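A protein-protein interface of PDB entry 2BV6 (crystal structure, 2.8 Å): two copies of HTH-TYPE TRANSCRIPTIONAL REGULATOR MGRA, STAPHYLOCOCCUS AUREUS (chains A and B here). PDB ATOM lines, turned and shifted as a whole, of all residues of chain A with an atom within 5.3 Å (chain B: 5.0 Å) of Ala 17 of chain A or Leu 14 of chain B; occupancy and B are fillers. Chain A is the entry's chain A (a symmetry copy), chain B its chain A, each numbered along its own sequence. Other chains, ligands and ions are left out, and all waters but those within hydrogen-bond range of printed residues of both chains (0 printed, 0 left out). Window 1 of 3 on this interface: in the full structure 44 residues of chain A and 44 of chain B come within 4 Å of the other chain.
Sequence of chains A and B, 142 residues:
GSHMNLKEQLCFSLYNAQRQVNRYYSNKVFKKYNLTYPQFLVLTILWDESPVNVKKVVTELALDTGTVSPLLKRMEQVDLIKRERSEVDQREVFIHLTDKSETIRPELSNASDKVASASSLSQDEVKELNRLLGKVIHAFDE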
ATOM      1  N   PHE A  12     -30.014  12.725 -22.256  1.00  0.00           N
ATOM      2  CA  PHE A  12     -28.703  12.726 -21.616  1.00  0.00           C
ATOM      3  C   PHE A  12     -28.183  14.141 -21.435  1.00  0.00           C
ATOM      4  O   PHE A  12     -27.577  14.461 -20.413  1.00  0.00           O
ATOM      5  CB  PHE A  12     -27.699  11.900 -22.431  1.00  0.00           C
ATOM      6  CG  PHE A  12     -27.946  10.413 -22.372  1.00  0.00           C
ATOM      7  CD1 PHE A  12     -28.826   9.799 -23.257  1.00  0.00           C
ATOM      8  CD2 PHE A  12     -27.322   9.629 -21.404  1.00  0.00           C
ATOM      9  CE1 PHE A  12     -29.084   8.424 -23.178  1.00  0.00           C
ATOM     10  CE2 PHE A  12     -27.573   8.255 -21.315  1.00  0.00           C
ATOM     11  CZ  PHE A  12     -28.456   7.653 -22.204  1.00  0.00           C
ATOM     12  N   SER A  13     -28.434  14.989 -22.426  1.00  0.00           N
ATOM     13  CA  SER A  13     -27.991  16.385 -22.384  1.00  0.00           C
ATOM     14  C   SER A  13     -28.566  17.146 -21.187  1.00  0.00           C
ATOM     15  O   SER A  13     -27.814  17.746 -20.411  1.00  0.00           O
ATOM     16  CB  SER A  13     -28.367  17.095 -23.690  1.00  0.00           C
ATOM     17  OG  SER A  13     -27.669  16.532 -24.794  1.00  0.00           O
ATOM     18  N   LEU A  14     -29.891  17.118 -21.042  1.00  0.00           N
ATOM     19  CA  LEU A  14     -30.568  17.788 -19.928  1.00  0.00           C
ATOM     20  C   LEU A  14     -30.097  17.252 -18.590  1.00  0.00           C
ATOM     21  O   LEU A  14     -29.654  18.003 -17.711  1.00  0.00           O
ATOM     22  CB  LEU A  14     -32.076  17.592 -20.031  1.00  0.00           C
ATOM     23  CG  LEU A  14     -32.709  18.439 -21.132  1.00  0.00           C
ATOM     24  CD1 LEU A  14     -34.160  18.043 -21.353  1.00  0.00           C
ATOM     25  CD2 LEU A  14     -32.582  19.899 -20.737  1.00  0.00           C
ATOM     26  N   TYR A  15     -30.210  15.940 -18.443  1.00  0.00           N
ATOM     27  CA  TYR A  15     -29.796  15.267 -17.229  1.00  0.00           C
ATOM     28  C   TYR A  15     -28.405  15.706 -16.811  1.00  0.00           C
ATOM     29  O   TYR A  15     -28.187  16.151 -15.686  1.00  0.00           O
ATOM     30  CB  TYR A  15     -29.777  13.762 -17.443  1.00  0.00           C
ATOM     31  CG  TYR A  15     -29.310  13.038 -16.224  1.00  0.00           C
ATOM     32  CD1 TYR A  15     -30.174  12.828 -15.157  1.00  0.00           C
ATOM     33  CD2 TYR A  15     -27.986  12.626 -16.097  1.00  0.00           C
ATOM     34  CE1 TYR A  15     -29.737  12.227 -13.990  1.00  0.00           C
ATOM     35  CE2 TYR A  15     -27.534  12.024 -14.926  1.00  0.00           C
ATOM     36  CZ  TYR A  15     -28.420  11.828 -13.878  1.00  0.00           C
ATOM     37  OH  TYR A  15     -28.006  11.231 -12.710  1.00  0.00           O
ATOM     38  N   ASN A  16     -27.462  15.573 -17.733  1.00  0.00           N
ATOM     39  CA  ASN A  16     -26.083  15.921 -17.454  1.00  0.00           C
ATOM     40  C   ASN A  16     -25.803  17.389 -17.219  1.00  0.00           C
ATOM     41  O   ASN A  16     -25.018  17.734 -16.329  1.00  0.00           O
ATOM     42  CB  ASN A  16     -25.174  15.393 -18.561  1.00  0.00           C
ATOM     43  CG  ASN A  16     -24.926  13.907 -18.432  1.00  0.00           C
ATOM     44  OD1 ASN A  16     -24.510  13.428 -17.372  1.00  0.00           O
ATOM     45  ND2 ASN A  16     -25.176  13.166 -19.507  1.00  0.00           N
ATOM     46  N   ALA A  17     -26.424  18.254 -18.012  1.00  0.00           N
ATOM     47  CA  ALA A  17     -26.216  19.683 -17.845  1.00  0.00           C
ATOM     48  C   ALA A  17     -26.530  20.058 -16.393  1.00  0.00           C
ATOM     49  O   ALA A  17     -25.660  20.542 -15.650  1.00  0.00           O
ATOM     50  CB  ALA A  17     -27.111  20.437 -18.790  1.00  0.00           C
ATOM     51  N   GLN A  18     -27.775  19.817 -15.993  1.00  0.00           N
ATOM     52  CA  GLN A  18     -28.213  20.110 -14.639  1.00  0.00           C
ATOM     53  C   GLN A  18     -27.281  19.419 -13.661  1.00  0.00           C
ATOM     54  O   GLN A  18     -26.706  20.047 -12.772  1.00  0.00           O
ATOM     55  CB  GLN A  18     -29.652  19.619 -14.449  1.00  0.00           C
ATOM     56  CG  GLN A  18     -30.189  19.645 -13.019  1.00  0.00           C
ATOM     57  CD  GLN A  18     -29.951  20.971 -12.304  1.00  0.00           C
ATOM     58  OE1 GLN A  18     -29.992  22.043 -12.920  1.00  0.00           O
ATOM     59  NE2 GLN A  18     -29.714  20.903 -10.990  1.00  0.00           N
ATOM     60  N   ARG A  19     -27.119  18.117 -13.846  1.00  0.00           N
ATOM     61  CA  ARG A  19     -26.267  17.321 -12.978  1.00  0.00           C
ATOM     62  C   ARG A  19     -24.913  17.996 -12.766  1.00  0.00           C
ATOM     63  O   ARG A  19     -24.408  18.078 -11.644  1.00  0.00           O
ATOM     64  CB  ARG A  19     -26.085  15.929 -13.583  1.00  0.00           C
ATOM     65  CG  ARG A  19     -25.472  14.906 -12.644  1.00  0.00           C
ATOM     66  CD  ARG A  19     -26.318  14.669 -11.408  1.00  0.00           C
ATOM     67  NE  ARG A  19     -25.683  13.686 -10.533  1.00  0.00           N
ATOM     68  CZ  ARG A  19     -26.179  13.290  -9.365  1.00  0.00           C
ATOM     69  NH1 ARG A  19     -27.327  13.797  -8.924  1.00  0.00           N
ATOM     70  NH2 ARG A  19     -25.528  12.388  -8.638  1.00  0.00           N
ATOM     71  N   GLN A  20     -24.340  18.496 -13.853  1.00  0.00           N
ATOM     72  CA  GLN A  20     -23.051  19.171 -13.791  1.00  0.00           C
ATOM     73  C   GLN A  20     -23.115  20.458 -12.988  1.00  0.00           C
ATOM     74  O   GLN A  20     -22.361  20.642 -12.026  1.00  0.00           O
ATOM     75  CB  GLN A  20     -22.544  19.465 -15.203  1.00  0.00           C
ATOM     76  CG  GLN A  20     -21.979  18.242 -15.880  1.00  0.00           C
ATOM     77  CD  GLN A  20     -20.969  17.547 -14.992  1.00  0.00           C
ATOM     78  OE1 GLN A  20     -19.938  18.124 -14.636  1.00  0.00           O
ATOM     79  NE2 GLN A  20     -21.270  16.310 -14.611  1.00  0.00           N
ATOM     80  N   VAL A  21     -24.021  21.346 -13.389  1.00  0.00           N
ATOM     81  CA  VAL A  21     -24.187  22.620 -12.707  1.00  0.00           C
ATOM     82  C   VAL A  21     -24.419  22.419 -11.207  1.00  0.00           C
ATOM     83  O   VAL A  21     -23.939  23.208 -10.387  1.00  0.00           O
ATOM     84  CB  VAL A  21     -25.369  23.405 -13.293  1.00  0.00           C
ATOM     85  CG1 VAL A  21     -25.452  24.765 -12.653  1.00  0.00           C
ATOM     86  CG2 VAL A  21     -25.210  23.531 -14.788  1.00  0.00           C
ATOM     87  N   ASN A  22     -25.153  21.372 -10.837  1.00  0.00           N
ATOM     88  CA  ASN A  22     -25.393  21.144  -9.422  1.00  0.00           C
ATOM     89  C   ASN A  22     -24.093  20.705  -8.792  1.00  0.00           C
ATOM     90  O   ASN A  22     -23.698  21.224  -7.746  1.00  0.00           O
ATOM     91  CB  ASN A  22     -26.466  20.082  -9.198  1.00  0.00           C
ATOM     92  CG  ASN A  22     -26.731  19.821  -7.712  1.00  0.00           C
ATOM     93  OD1 ASN A  22     -27.798  19.334  -7.341  1.00  0.00           O
ATOM     94  ND2 ASN A  22     -25.759  20.133  -6.861  1.00  0.00           N
ATOM     95  N   VAL A 115     -22.406  30.646 -14.326  1.00  0.00           N
ATOM     96  CA  VAL A 115     -22.666  29.533 -15.222  1.00  0.00           C
ATOM     97  C   VAL A 115     -22.454  29.974 -16.660  1.00  0.00           C
ATOM     98  O   VAL A 115     -21.498  29.558 -17.304  1.00  0.00           O
ATOM     99  CB  VAL A 115     -24.121  29.015 -15.049  1.00  0.00           C
ATOM    100  CG1 VAL A 115     -24.502  28.103 -16.201  1.00  0.00           C
ATOM    101  CG2 VAL A 115     -24.253  28.266 -13.731  1.00  0.00           C
ATOM    102  N   LEU A 133     -35.213  25.521 -23.548  1.00  0.00           N
ATOM    103  CA  LEU A 133     -35.550  24.888 -22.282  1.00  0.00           C
ATOM    104  C   LEU A 133     -37.003  25.204 -21.941  1.00  0.00           C
ATOM    105  O   LEU A 133     -37.726  24.360 -21.400  1.00  0.00           O
ATOM    106  CB  LEU A 133     -34.624  25.389 -21.170  1.00  0.00           C
ATOM    107  CG  LEU A 133     -33.218  24.786 -21.205  1.00  0.00           C
ATOM    108  CD1 LEU A 133     -32.338  25.404 -20.133  1.00  0.00           C
ATOM    109  CD2 LEU A 133     -33.323  23.286 -20.995  1.00  0.00           C
ATOM    110  N   LEU B  10     -31.014  30.698 -16.262  1.00  0.00           N
ATOM    111  CA  LEU B  10     -30.574  29.376 -16.685  1.00  0.00           C
ATOM    112  C   LEU B  10     -30.694  28.386 -15.543  1.00  0.00           C
ATOM    113  O   LEU B  10     -31.166  27.259 -15.723  1.00  0.00           O
ATOM    114  CB  LEU B  10     -29.117  29.417 -17.136  1.00  0.00           C
ATOM    115  CG  LEU B  10     -28.828  29.591 -18.621  1.00  0.00           C
ATOM    116  CD1 LEU B  10     -27.324  29.502 -18.816  1.00  0.00           C
ATOM    117  CD2 LEU B  10     -29.536  28.514 -19.434  1.00  0.00           C
ATOM    118  N   CYS B  11     -30.247  28.810 -14.369  1.00  0.00           N
ATOM    119  CA  CYS B  11     -30.317  27.949 -13.219  1.00  0.00           C
ATOM    120  C   CYS B  11     -31.711  27.376 -13.073  1.00  0.00           C
ATOM    121  O   CYS B  11     -31.863  26.176 -12.858  1.00  0.00           O
ATOM    122  CB  CYS B  11     -29.906  28.709 -11.970  1.00  0.00           C
ATOM    123  SG  CYS B  11     -28.108  28.797 -11.786  1.00  0.00           S
ATOM    124  N   PHE B  12     -32.727  28.221 -13.216  1.00  0.00           N
ATOM    125  CA  PHE B  12     -34.109  27.767 -13.100  1.00  0.00           C
ATOM    126  C   PHE B  12     -34.531  26.979 -14.328  1.00  0.00           C
ATOM    127  O   PHE B  12     -35.242  25.981 -14.219  1.00  0.00           O
ATOM    128  CB  PHE B  12     -35.057  28.955 -12.889  1.00  0.00           C
ATOM    129  CG  PHE B  12     -34.942  29.589 -11.525  1.00  0.00           C
ATOM    130  CD1 PHE B  12     -34.003  30.584 -11.276  1.00  0.00           C
ATOM    131  CD2 PHE B  12     -35.754  29.163 -10.476  1.00  0.00           C
ATOM    132  CE1 PHE B  12     -33.871  31.146 -10.000  1.00  0.00           C
ATOM    133  CE2 PHE B  12     -35.630  29.717  -9.197  1.00  0.00           C
ATOM    134  CZ  PHE B  12     -34.686  30.710  -8.959  1.00  0.00           C
ATOM    135  N   SER B  13     -34.079  27.425 -15.495  1.00  0.00           N
ATOM    136  CA  SER B  13     -34.408  26.762 -16.759  1.00  0.00           C
ATOM    137  C   SER B  13     -33.942  25.305 -16.795  1.00  0.00           C
ATOM    138  O   SER B  13     -34.741  24.401 -17.065  1.00  0.00           O
ATOM    139  CB  SER B  13     -33.802  27.539 -17.934  1.00  0.00           C
ATOM    140  OG  SER B  13     -34.387  28.831 -18.044  1.00  0.00           O
ATOM    141  N   LEU B  14     -32.656  25.083 -16.523  1.00  0.00           N
ATOM    142  CA  LEU B  14     -32.084  23.734 -16.505  1.00  0.00           C
ATOM    143  C   LEU B  14     -32.775  22.854 -15.480  1.00  0.00           C
ATOM    144  O   LEU B  14     -33.270  21.763 -15.793  1.00  0.00           O
ATOM    145  CB  LEU B  14     -30.597  23.793 -16.175  1.00  0.00           C
ATOM    146  CG  LEU B  14     -29.753  24.305 -17.339  1.00  0.00           C
ATOM    147  CD1 LEU B  14     -28.323  24.569 -16.897  1.00  0.00           C
ATOM    148  CD2 LEU B  14     -29.813  23.276 -18.454  1.00  0.00           C
ATOM    149  N   TYR B  15     -32.790  23.338 -14.247  1.00  0.00           N
ATOM    150  CA  TYR B  15     -33.419  22.627 -13.153  1.00  0.00           C
ATOM    151  C   TYR B  15     -34.813  22.166 -13.534  1.00  0.00           C
ATOM    152  O   TYR B  15     -35.145  20.986 -13.434  1.00  0.00           O
ATOM    153  CB  TYR B  15     -33.531  23.531 -11.935  1.00  0.00           C
ATOM    154  CG  TYR B  15     -34.217  22.844 -10.801  1.00  0.00           C
ATOM    155  CD1 TYR B  15     -33.527  21.937 -10.007  1.00  0.00           C
ATOM    156  CD2 TYR B  15     -35.575  23.036 -10.562  1.00  0.00           C
ATOM    157  CE1 TYR B  15     -34.165  21.235  -9.000  1.00  0.00           C
ATOM    158  CE2 TYR B  15     -36.231  22.332  -9.555  1.00  0.00           C
ATOM    159  CZ  TYR B  15     -35.514  21.434  -8.779  1.00  0.00           C
ATOM    160  OH  TYR B  15     -36.130  20.727  -7.772  1.00  0.00           O
ATOM    161  N   ASN B  16     -35.630  23.114 -13.971  1.00  0.00           N
ATOM    162  CA  ASN B  16     -37.001  22.816 -14.335  1.00  0.00           C
ATOM    163  C   ASN B  16     -37.189  21.937 -15.552  1.00  0.00           C
ATOM    164  O   ASN B  16     -38.057  21.058 -15.550  1.00  0.00           O
ATOM    165  CB  ASN B  16     -37.791  24.112 -14.507  1.00  0.00           C
ATOM    166  CG  ASN B  16     -38.175  24.724 -13.179  1.00  0.00           C
ATOM    167  OD1 ASN B  16     -38.769  24.056 -12.326  1.00  0.00           O
ATOM    168  ND2 ASN B  16     -37.842  25.998 -12.992  1.00  0.00           N
ATOM    169  N   ALA B  17     -36.398  22.171 -16.591  1.00  0.00           N
ATOM    170  CA  ALA B  17     -36.509  21.364 -17.795  1.00  0.00           C
ATOM    171  C   ALA B  17     -36.367  19.887 -17.411  1.00  0.00           C
ATOM    172  O   ALA B  17     -37.287  19.078 -17.610  1.00  0.00           O
ATOM    173  CB  ALA B  17     -35.436  21.761 -18.770  1.00  0.00           C
ATOM    174  N   GLN B  18     -35.211  19.550 -16.846  1.00  0.00           N
ATOM    175  CA  GLN B  18     -34.939  18.189 -16.418  1.00  0.00           C
ATOM    176  C   GLN B  18     -36.049  17.735 -15.486  1.00  0.00           C
ATOM    177  O   GLN B  18     -36.686  16.705 -15.705  1.00  0.00           O
ATOM    178  CB  GLN B  18     -33.584  18.137 -15.704  1.00  0.00           C
ATOM    179  CG  GLN B  18     -33.247  16.828 -14.993  1.00  0.00           C
ATOM    180  CD  GLN B  18     -33.471  15.591 -15.857  1.00  0.00           C
ATOM    181  OE1 GLN B  18     -33.259  15.619 -17.076  1.00  0.00           O
ATOM    182  NE2 GLN B  18     -33.889  14.491 -15.223  1.00  0.00           N
ATOM    183  N   ARG B  19     -36.290  18.529 -14.453  1.00  0.00           N
ATOM    184  CA  ARG B  19     -37.314  18.214 -13.470  1.00  0.00           C
ATOM    185  C   ARG B  19     -38.624  17.819 -14.148  1.00  0.00           C
ATOM    186  O   ARG B  19     -39.269  16.838 -13.771  1.00  0.00           O
ATOM    187  CB  ARG B  19     -37.525  19.420 -12.555  1.00  0.00           C
ATOM    188  CG  ARG B  19     -38.342  19.132 -11.307  1.00  0.00           C
ATOM    189  CD  ARG B  19     -37.693  18.092 -10.414  1.00  0.00           C
ATOM    190  NE  ARG B  19     -38.519  17.843  -9.235  1.00  0.00           N
ATOM    191  CZ  ARG B  19     -38.221  16.967  -8.281  1.00  0.00           C
ATOM    192  NH1 ARG B  19     -37.107  16.247  -8.365  1.00  0.00           N
ATOM    193  NH2 ARG B  19     -39.036  16.812  -7.243  1.00  0.00           N
ATOM    194  N   LEU B 133     -26.374  22.859 -24.322  1.00  0.00           N
ATOM    195  CA  LEU B 133     -26.266  22.021 -23.137  1.00  0.00           C
ATOM    196  C   LEU B 133     -24.852  21.455 -23.058  1.00  0.00           C
ATOM    197  O   LEU B 133     -24.280  21.321 -21.970  1.00  0.00           O
ATOM    198  CB  LEU B 133     -27.290  20.885 -23.188  1.00  0.00           C
ATOM    199  CG  LEU B 133     -28.723  21.316 -22.867  1.00  0.00           C
ATOM    200  CD1 LEU B 133     -29.687  20.156 -23.033  1.00  0.00           C
ATOM    201  CD2 LEU B 133     -28.771  21.835 -21.441  1.00  0.00           C
ATOM    202  N   VAL B 136     -22.609  23.781 -21.427  1.00  0.00           N
ATOM    203  CA  VAL B 136     -22.900  23.821 -19.994  1.00  0.00           C
ATOM    204  C   VAL B 136     -22.214  22.652 -19.294  1.00  0.00           C
ATOM    205  O   VAL B 136     -21.621  22.804 -18.221  1.00  0.00           O
ATOM    206  CB  VAL B 136     -24.424  23.708 -19.726  1.00  0.00           C
ATOM    207  CG1 VAL B 136     -24.709  23.923 -18.250  1.00  0.00           C
ATOM    208  CG2 VAL B 136     -25.190  24.712 -20.581  1.00  0.00           C
ATOM    209  N   ILE B 137     -22.303  21.485 -19.923  1.00  0.00           N
ATOM    210  CA  ILE B 137     -21.733  20.264 -19.389  1.00  0.00           C
ATOM    211  C   ILE B 137     -20.236  20.327 -19.132  1.00  0.00           C
ATOM    212  O   ILE B 137     -19.795  20.123 -18.003  1.00  0.00           O
ATOM    213  CB  ILE B 137     -22.060  19.088 -20.312  1.00  0.00           C
ATOM    214  CG1 ILE B 137     -23.581  18.924 -20.378  1.00  0.00           C
ATOM    215  CG2 ILE B 137     -21.412  17.826 -19.796  1.00  0.00           C
ATOM    216  CD1 ILE B 137     -24.077  17.755 -21.203  1.00  0.00           C
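N of Tyr 15 of chain B lies within hydrogen-bond range of OE1 of Gln 18 of chain A, at 3.4 Å. The side-chain amide oxygen of Gln 18 of chain B lies within hydrogen-bond range of the backbone NH of Tyr 15 of chain A, at 3.4 Å.
O of Phe 12 of chain A lies within hydrogen-bond range of ND2 of Asn 16 of chain A, 2.9 Å away.
Among the printed residues, merely in contact across the chains: Leu 133 of chain A with Ser 13 of chain B, Ser 13 of chain A with Leu 133 of chain B, Ala 17 of chain A with Leu 133 of chain B, Leu 133 of chain A with Ala 17 of chain B, Val 21 of chain A with Val 136 of chain B, Gln 20 of chain A with Ile 137 of chain B, Leu 14 of chain A with Leu 133 of chain B, Leu 133 of chain A with Leu 14 of chain B, Asn 16 of chain A with Ile 137 of chain B, Ala 17 of chain A with Ile 137 of chain B, Gln 18 of chain A with Leu 14 of chain B, Leu 14 of chain A with Gln 18 of chain B, Ser 13 of chain A with Ile 137 of chain B, Val 21 of chain A with Leu 14 of chain B, Ala 17 of chain A with Leu 14 of chain B and Leu 14 of chain A with Ala 17 of chain B.
Of the printed residues of chain B, Leu 14 of chain A touches Ala 17 (3.9 Å), Gln 18 (3.7 Å) and Leu 133 (3.6 Å). Of the printed residues of chain B, Ala 17 of chain A touches Leu 14 (3.9 Å), Leu 133 (3.4 Å) and Ile 137 (3.7 Å). Phe 12 of chain B touches none of the printed residues of chain A. Of the printed residues of chain A, Ser 13 of chain B touches Leu 133. Leu 14 of chain B touches four residues of chain A. The nearest residue of chain A that does not touch Leu 14 of chain B is Leu 14 of chain A (4.9 Å).
Printed residues of chain B that touch a printed residue of chain A: Ser 13, Leu 14, Tyr 15, Ala 17, Gln 18, Leu 133, Val 136 and Ile 137. Hydrophobic or aromatic side chains of chain B that line the printed part of chain A: Leu 14, Tyr 15, Ala 17, Leu 133, Val 136 and Ile 137. Printed residues of chain A that touch a printed residue of chain B: Ser 13, Leu 14, Tyr 15, Asn 16, Ala 17, Gln 18, Gln 20, Val 21 and Leu 133. Among the printed residues, 18 pairs touch across the chains.
Ser 13 of chain A touches Leu 133 of chain B, and with the chains exchanged Leu 133 of chain A touches Ser 13 of chain B. Leu 14 of chain A touches Ala 17 of chain B, and with the chains exchanged Ala 17 of chain A touches Leu 14 of chain B. Tyr 15 of chain A touches Gln 18 of chain B, and with the chains exchanged Gln 18 of chain A touches Tyr 15 of chain B. Ala 17 of chain A touches Leu 133 of chain B, and with the chains exchanged Leu 133 of chain A touches Ala 17 of chain B. Positions printed for both chains: 12, 13, 14, 15, 16, 17, 18, 19 and 133. Of the 18 pairs that touch across the chains among the printed residues, 12 have their exchanged pair printed and touching as well.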
